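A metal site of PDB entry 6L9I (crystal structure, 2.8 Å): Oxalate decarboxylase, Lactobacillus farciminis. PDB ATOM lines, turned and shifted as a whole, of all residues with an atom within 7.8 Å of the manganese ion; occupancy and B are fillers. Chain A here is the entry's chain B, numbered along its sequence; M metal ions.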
ATOM      1  N   ALA A 239       1.359  10.319  -5.221  1.00  0.00           N
ATOM      2  CA  ALA A 239       1.665  11.746  -5.212  1.00  0.00           C
ATOM      3  C   ALA A 239       1.443  12.285  -6.619  1.00  0.00           C
ATOM      4  O   ALA A 239       1.958  11.719  -7.591  1.00  0.00           O
ATOM      5  CB  ALA A 239       3.098  12.011  -4.769  1.00  0.00           C
ATOM      6  N   VAL A 241       2.337  15.249  -8.944  1.00  0.00           N
ATOM      7  CA  VAL A 241       3.413  16.226  -8.988  1.00  0.00           C
ATOM      8  C   VAL A 241       3.188  17.107 -10.198  1.00  0.00           C
ATOM      9  O   VAL A 241       2.983  16.621 -11.321  1.00  0.00           O
ATOM     10  CB  VAL A 241       4.799  15.547  -9.081  1.00  0.00           C
ATOM     11  CG1 VAL A 241       5.904  16.599  -8.980  1.00  0.00           C
ATOM     12  CG2 VAL A 241       4.951  14.503  -7.975  1.00  0.00           C
ATOM     13  N   ARG A 249      12.167  17.981 -10.269  1.00  0.00           N
ATOM     14  CA  ARG A 249      11.979  17.191  -9.047  1.00  0.00           C
ATOM     15  C   ARG A 249      13.369  16.823  -8.551  1.00  0.00           C
ATOM     16  O   ARG A 249      14.077  16.049  -9.202  1.00  0.00           O
ATOM     17  CB  ARG A 249      11.129  15.957  -9.310  1.00  0.00           C
ATOM     18  CG  ARG A 249      10.742  15.174  -8.058  1.00  0.00           C
ATOM     19  CD  ARG A 249       9.548  15.797  -7.345  1.00  0.00           C
ATOM     20  NE  ARG A 249       8.718  14.792  -6.685  1.00  0.00           N
ATOM     21  CZ  ARG A 249       8.934  14.326  -5.453  1.00  0.00           C
ATOM     22  NH1 ARG A 249       9.964  14.784  -4.744  1.00  0.00           N
ATOM     23  NH2 ARG A 249       8.129  13.410  -4.939  1.00  0.00           N
ATOM     24  N   GLU A 250      13.775  17.378  -7.416  1.00  0.00           N
ATOM     25  CA  GLU A 250      15.155  17.286  -6.982  1.00  0.00           C
ATOM     26  C   GLU A 250      15.550  15.826  -6.736  1.00  0.00           C
ATOM     27  O   GLU A 250      14.708  14.938  -6.570  1.00  0.00           O
ATOM     28  CB  GLU A 250      15.371  18.115  -5.724  1.00  0.00           C
ATOM     29  CG  GLU A 250      14.386  17.808  -4.608  1.00  0.00           C
ATOM     30  CD  GLU A 250      14.941  18.173  -3.248  1.00  0.00           C
ATOM     31  OE1 GLU A 250      16.145  17.966  -3.021  1.00  0.00           O
ATOM     32  OE2 GLU A 250      14.151  18.657  -2.403  1.00  0.00           O
ATOM     33  N   HIS A 252      16.311  12.532  -5.234  1.00  0.00           N
ATOM     34  CA  HIS A 252      15.676  11.941  -4.071  1.00  0.00           C
ATOM     35  C   HIS A 252      15.531  10.448  -4.296  1.00  0.00           C
ATOM     36  O   HIS A 252      15.770   9.929  -5.383  1.00  0.00           O
ATOM     37  CB  HIS A 252      14.294  12.569  -3.822  1.00  0.00           C
ATOM     38  CG  HIS A 252      13.272  12.182  -4.849  1.00  0.00           C
ATOM     39  ND1 HIS A 252      13.292  12.657  -6.142  1.00  0.00           N
ATOM     40  CD2 HIS A 252      12.214  11.344  -4.769  1.00  0.00           C
ATOM     41  CE1 HIS A 252      12.277  12.146  -6.808  1.00  0.00           C
ATOM     42  NE2 HIS A 252      11.599  11.347  -6.002  1.00  0.00           N
ATOM     43  N   TRP A 253      15.111   9.743  -3.241  1.00  0.00           N
ATOM     44  CA  TRP A 253      14.742   8.352  -3.385  1.00  0.00           C
ATOM     45  C   TRP A 253      13.646   8.017  -2.396  1.00  0.00           C
ATOM     46  O   TRP A 253      13.414   8.733  -1.419  1.00  0.00           O
ATOM     47  CB  TRP A 253      15.955   7.423  -3.212  1.00  0.00           C
ATOM     48  CG  TRP A 253      16.431   7.261  -1.795  1.00  0.00           C
ATOM     49  CD1 TRP A 253      15.964   6.390  -0.867  1.00  0.00           C
ATOM     50  CD2 TRP A 253      17.499   7.988  -1.162  1.00  0.00           C
ATOM     51  NE1 TRP A 253      16.657   6.520   0.313  1.00  0.00           N
ATOM     52  CE2 TRP A 253      17.608   7.492   0.154  1.00  0.00           C
ATOM     53  CE3 TRP A 253      18.374   8.997  -1.576  1.00  0.00           C
ATOM     54  CZ2 TRP A 253      18.550   7.983   1.064  1.00  0.00           C
ATOM     55  CZ3 TRP A 253      19.304   9.483  -0.671  1.00  0.00           C
ATOM     56  CH2 TRP A 253      19.385   8.978   0.622  1.00  0.00           C
ATOM     57  N   HIS A 254      12.978   6.892  -2.660  1.00  0.00           N
ATOM     58  CA  HIS A 254      11.936   6.396  -1.771  1.00  0.00           C
ATOM     59  C   HIS A 254      12.460   5.161  -1.049  1.00  0.00           C
ATOM     60  O   HIS A 254      12.763   4.148  -1.687  1.00  0.00           O
ATOM     61  CB  HIS A 254      10.673   6.070  -2.563  1.00  0.00           C
ATOM     62  CG  HIS A 254      10.194   7.211  -3.414  1.00  0.00           C
ATOM     63  ND1 HIS A 254       9.296   8.158  -2.972  1.00  0.00           N
ATOM     64  CD2 HIS A 254      10.503   7.555  -4.690  1.00  0.00           C
ATOM     65  CE1 HIS A 254       9.065   9.029  -3.931  1.00  0.00           C
ATOM     66  NE2 HIS A 254       9.786   8.687  -4.989  1.00  0.00           N
ATOM     67  N   GLU A 259       8.772   2.721  -7.505  1.00  0.00           N
ATOM     68  CA  GLU A 259       7.884   3.811  -7.911  1.00  0.00           C
ATOM     69  C   GLU A 259       7.374   3.585  -9.329  1.00  0.00           C
ATOM     70  O   GLU A 259       8.134   3.164 -10.205  1.00  0.00           O
ATOM     71  CB  GLU A 259       8.592   5.160  -7.807  1.00  0.00           C
ATOM     72  CG  GLU A 259       7.866   6.302  -8.492  1.00  0.00           C
ATOM     73  CD  GLU A 259       8.603   7.615  -8.340  1.00  0.00           C
ATOM     74  OE1 GLU A 259       9.433   7.721  -7.418  1.00  0.00           O
ATOM     75  OE2 GLU A 259       8.367   8.538  -9.148  1.00  0.00           O
ATOM     76  N   TRP A 260       6.092   3.875  -9.544  1.00  0.00           N
ATOM     77  CA  TRP A 260       5.404   3.684 -10.825  1.00  0.00           C
ATOM     78  C   TRP A 260       4.796   5.011 -11.247  1.00  0.00           C
ATOM     79  O   TRP A 260       4.003   5.593 -10.502  1.00  0.00           O
ATOM     80  CB  TRP A 260       4.331   2.609 -10.680  1.00  0.00           C
ATOM     81  CG  TRP A 260       3.630   2.189 -11.933  1.00  0.00           C
ATOM     82  CD1 TRP A 260       3.909   1.077 -12.683  1.00  0.00           C
ATOM     83  CD2 TRP A 260       2.525   2.836 -12.567  1.00  0.00           C
ATOM     84  NE1 TRP A 260       3.046   1.011 -13.754  1.00  0.00           N
ATOM     85  CE2 TRP A 260       2.195   2.076 -13.702  1.00  0.00           C
ATOM     86  CE3 TRP A 260       1.792   3.994 -12.282  1.00  0.00           C
ATOM     87  CZ2 TRP A 260       1.144   2.437 -14.565  1.00  0.00           C
ATOM     88  CZ3 TRP A 260       0.764   4.351 -13.136  1.00  0.00           C
ATOM     89  CH2 TRP A 260       0.454   3.574 -14.263  1.00  0.00           C
ATOM     90  N   ASP A 261       5.139   5.490 -12.432  1.00  0.00           N
ATOM     91  CA  ASP A 261       4.755   6.820 -12.875  1.00  0.00           C
ATOM     92  C   ASP A 261       3.798   6.744 -14.055  1.00  0.00           C
ATOM     93  O   ASP A 261       3.973   5.919 -14.952  1.00  0.00           O
ATOM     94  CB  ASP A 261       5.958   7.651 -13.301  1.00  0.00           C
ATOM     95  CG  ASP A 261       7.044   7.671 -12.277  1.00  0.00           C
ATOM     96  OD1 ASP A 261       6.760   8.036 -11.118  1.00  0.00           O
ATOM     97  OD2 ASP A 261       8.183   7.313 -12.631  1.00  0.00           O
ATOM     98  N   ILE A 292      10.702   3.510 -11.480  1.00  0.00           N
ATOM     99  CA  ILE A 292      11.961   3.746 -10.775  1.00  0.00           C
ATOM    100  C   ILE A 292      12.186   2.576  -9.839  1.00  0.00           C
ATOM    101  O   ILE A 292      11.334   2.296  -8.981  1.00  0.00           O
ATOM    102  CB  ILE A 292      11.957   5.074 -10.005  1.00  0.00           C
ATOM    103  CG1 ILE A 292      11.997   6.255 -10.973  1.00  0.00           C
ATOM    104  CG2 ILE A 292      13.161   5.144  -9.073  1.00  0.00           C
ATOM    105  CD1 ILE A 292      10.690   6.973 -11.074  1.00  0.00           C
ATOM    106  N   ALA A 296      16.076   3.468  -5.702  1.00  0.00           N
ATOM    107  CA  ALA A 296      16.953   4.051  -6.702  1.00  0.00           C
ATOM    108  C   ALA A 296      16.931   5.575  -6.607  1.00  0.00           C
ATOM    109  O   ALA A 296      15.890   6.180  -6.361  1.00  0.00           O
ATOM    110  CB  ALA A 296      16.523   3.619  -8.106  1.00  0.00           C
ATOM    111  N   HIS A 298      16.987   9.303  -8.095  1.00  0.00           N
ATOM    112  CA  HIS A 298      16.518   9.788  -9.384  1.00  0.00           C
ATOM    113  C   HIS A 298      16.147  11.259  -9.313  1.00  0.00           C
ATOM    114  O   HIS A 298      15.964  11.827  -8.236  1.00  0.00           O
ATOM    115  CB  HIS A 298      15.340   8.951  -9.902  1.00  0.00           C
ATOM    116  CG  HIS A 298      14.218   8.829  -8.926  1.00  0.00           C
ATOM    117  ND1 HIS A 298      14.257   7.981  -7.841  1.00  0.00           N
ATOM    118  CD2 HIS A 298      13.008   9.440  -8.884  1.00  0.00           C
ATOM    119  CE1 HIS A 298      13.127   8.088  -7.165  1.00  0.00           C
ATOM    120  NE2 HIS A 298      12.354   8.961  -7.772  1.00  0.00           N
ATOM    121  N   TYR A 299      16.055  11.854 -10.500  1.00  0.00           N
ATOM    122  CA  TYR A 299      15.505  13.198 -10.679  1.00  0.00           C
ATOM    123  C   TYR A 299      14.559  13.221 -11.868  1.00  0.00           C
ATOM    124  O   TYR A 299      14.684  12.412 -12.803  1.00  0.00           O
ATOM    125  CB  TYR A 299      16.607  14.242 -10.893  1.00  0.00           C
ATOM    126  CG  TYR A 299      17.356  14.020 -12.183  1.00  0.00           C
ATOM    127  CD1 TYR A 299      18.378  13.080 -12.247  1.00  0.00           C
ATOM    128  CD2 TYR A 299      17.011  14.695 -13.342  1.00  0.00           C
ATOM    129  CE1 TYR A 299      19.066  12.862 -13.418  1.00  0.00           C
ATOM    130  CE2 TYR A 299      17.683  14.473 -14.531  1.00  0.00           C
ATOM    131  CZ  TYR A 299      18.707  13.553 -14.557  1.00  0.00           C
ATOM    132  OH  TYR A 299      19.390  13.306 -15.729  1.00  0.00           O
ATOM    133  N   ILE A 300      13.642  14.190 -11.858  1.00  0.00           N
ATOM    134  CA  ILE A 300      12.648  14.414 -12.901  1.00  0.00           C
ATOM    135  C   ILE A 300      12.672  15.893 -13.232  1.00  0.00           C
ATOM    136  O   ILE A 300      12.222  16.720 -12.425  1.00  0.00           O
ATOM    137  CB  ILE A 300      11.247  13.972 -12.480  1.00  0.00           C
ATOM    138  CG1 ILE A 300      11.263  12.549 -11.919  1.00  0.00           C
ATOM    139  CG2 ILE A 300      10.265  14.113 -13.635  1.00  0.00           C
ATOM    140  CD1 ILE A 300       9.885  11.955 -11.721  1.00  0.00           C
ATOM    141  N   PHE A 310       2.402  14.587 -13.383  1.00  0.00           N
ATOM    142  CA  PHE A 310       2.509  13.132 -13.391  1.00  0.00           C
ATOM    143  C   PHE A 310       2.143  12.562 -12.017  1.00  0.00           C
ATOM    144  O   PHE A 310       2.019  13.290 -11.038  1.00  0.00           O
ATOM    145  CB  PHE A 310       3.906  12.666 -13.821  1.00  0.00           C
ATOM    146  CG  PHE A 310       5.017  13.184 -12.960  1.00  0.00           C
ATOM    147  CD1 PHE A 310       5.577  14.426 -13.193  1.00  0.00           C
ATOM    148  CD2 PHE A 310       5.519  12.418 -11.907  1.00  0.00           C
ATOM    149  CE1 PHE A 310       6.590  14.911 -12.404  1.00  0.00           C
ATOM    150  CE2 PHE A 310       6.542  12.894 -11.115  1.00  0.00           C
ATOM    151  CZ  PHE A 310       7.076  14.141 -11.370  1.00  0.00           C
ATOM    152  N   GLU A 312       3.349   9.766  -9.204  1.00  0.00           N
ATOM    153  CA  GLU A 312       4.203   8.779  -8.554  1.00  0.00           C
ATOM    154  C   GLU A 312       3.281   7.902  -7.721  1.00  0.00           C
ATOM    155  O   GLU A 312       2.625   8.384  -6.801  1.00  0.00           O
ATOM    156  CB  GLU A 312       5.242   9.448  -7.647  1.00  0.00           C
ATOM    157  CG  GLU A 312       5.986  10.635  -8.255  1.00  0.00           C
ATOM    158  CD  GLU A 312       7.097  11.158  -7.357  1.00  0.00           C
ATOM    159  OE1 GLU A 312       6.831  11.470  -6.185  1.00  0.00           O
ATOM    160  OE2 GLU A 312       8.247  11.262  -7.837  1.00  0.00           O
ATOM    161  N   VAL A 313       3.237   6.612  -8.029  1.00  0.00           N
ATOM    162  CA  VAL A 313       2.325   5.670  -7.394  1.00  0.00           C
ATOM    163  C   VAL A 313       3.147   4.546  -6.791  1.00  0.00           C
ATOM    164  O   VAL A 313       4.171   4.143  -7.354  1.00  0.00           O
ATOM    165  CB  VAL A 313       1.302   5.125  -8.419  1.00  0.00           C
ATOM    166  CG1 VAL A 313       0.266   4.258  -7.746  1.00  0.00           C
ATOM    167  CG2 VAL A 313       0.637   6.289  -9.162  1.00  0.00           C
ATOM    168  N   PHE A 314       2.700   4.056  -5.638  1.00  0.00           N
ATOM    169  CA  PHE A 314       3.472   3.082  -4.871  1.00  0.00           C
ATOM    170  C   PHE A 314       2.544   2.058  -4.253  1.00  0.00           C
ATOM    171  O   PHE A 314       1.435   2.379  -3.807  1.00  0.00           O
ATOM    172  CB  PHE A 314       4.287   3.755  -3.752  1.00  0.00           C
ATOM    173  CG  PHE A 314       4.939   5.047  -4.136  1.00  0.00           C
ATOM    174  CD1 PHE A 314       4.249   6.251  -4.063  1.00  0.00           C
ATOM    175  CD2 PHE A 314       6.261   5.072  -4.557  1.00  0.00           C
ATOM    176  CE1 PHE A 314       4.865   7.439  -4.411  1.00  0.00           C
ATOM    177  CE2 PHE A 314       6.877   6.261  -4.905  1.00  0.00           C
ATOM    178  CZ  PHE A 314       6.172   7.446  -4.837  1.00  0.00           C
ATOM    179  N   TYR A 319       3.178   7.165   2.050  1.00  0.00           N
ATOM    180  CA  TYR A 319       4.159   7.799   1.174  1.00  0.00           C
ATOM    181  C   TYR A 319       5.371   8.216   2.000  1.00  0.00           C
ATOM    182  O   TYR A 319       5.242   8.681   3.135  1.00  0.00           O
ATOM    183  CB  TYR A 319       3.557   9.002   0.454  1.00  0.00           C
ATOM    184  CG  TYR A 319       4.591   9.789  -0.342  1.00  0.00           C
ATOM    185  CD1 TYR A 319       5.367  10.768   0.278  1.00  0.00           C
ATOM    186  CD2 TYR A 319       4.808   9.543  -1.694  1.00  0.00           C
ATOM    187  CE1 TYR A 319       6.320  11.470  -0.425  1.00  0.00           C
ATOM    188  CE2 TYR A 319       5.761  10.252  -2.403  1.00  0.00           C
ATOM    189  CZ  TYR A 319       6.509  11.213  -1.755  1.00  0.00           C
ATOM    190  OH  TYR A 319       7.462  11.922  -2.464  1.00  0.00           O
ATOM    191  N   SER A 320       6.547   8.035   1.417  1.00  0.00           N
ATOM    192  CA  SER A 320       7.783   8.464   2.055  1.00  0.00           C
ATOM    193  C   SER A 320       8.824   8.718   0.978  1.00  0.00           C
ATOM    194  O   SER A 320       8.845   8.036  -0.058  1.00  0.00           O
ATOM    195  CB  SER A 320       8.286   7.428   3.056  1.00  0.00           C
ATOM    196  OG  SER A 320       8.816   6.288   2.399  1.00  0.00           O
ATOM    197  N   ASP A 321       9.667   9.710   1.223  1.00  0.00           N
ATOM    198  CA  ASP A 321      10.833   9.906   0.373  1.00  0.00           C
ATOM    199  C   ASP A 321      11.931  10.578   1.184  1.00  0.00           C
ATOM    200  O   ASP A 321      11.703  11.000   2.326  1.00  0.00           O
ATOM    201  CB  ASP A 321      10.496  10.707  -0.903  1.00  0.00           C
ATOM    202  CG  ASP A 321      10.344  12.216  -0.658  1.00  0.00           C
ATOM    203  OD1 ASP A 321      10.392  12.695   0.505  1.00  0.00           O
ATOM    204  OD2 ASP A 321      10.155  12.939  -1.656  1.00  0.00           O
HETATM  205 MN    MN M   1      10.189   9.673  -6.866  1.00  0.00          MN
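ND1 of His 252 lies within hydrogen-bond range of O of Glu 250, at 2.7 Å. The side-chain carboxylate (OE2) of Glu 259 lies close to the side-chain carboxylate (OD1) of Asp 261 (2.6 Å). O of Glu 312 sits at hydrogen-bond distance from N of Ala 239. OE1 of Glu 312 lies within salt-bridge range of NH2 of Arg 249 (2.6 Å). ND1 of His 254 lies within hydrogen-bond range of O of Ser 320 (3.0 Å). O of Ala 296 sits at hydrogen-bond distance from ND1 of His 298. The backbone NH of Ile 292 is in hydrogen-bond range of the backbone carbonyl oxygen of Glu 259, 2.9 Å away.
Within 4 Å of the manganese ion: His 252, His 254, Glu 259, His 298 and Glu 312. The nearest printed residue that does not touch the manganese ion is Arg 249 (4.7 Å).
The manganese ion is bound by a ring nitrogen (NE2) of His 254 (2.2 Å), the side-chain carboxylate of Glu 259 (2.2 Å), a ring nitrogen (NE2) of His 252 (2.4 Å), a ring nitrogen (NE2) of His 298 (2.5 Å) and the side-chain carboxylate of Glu 312 (2.7 Å).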
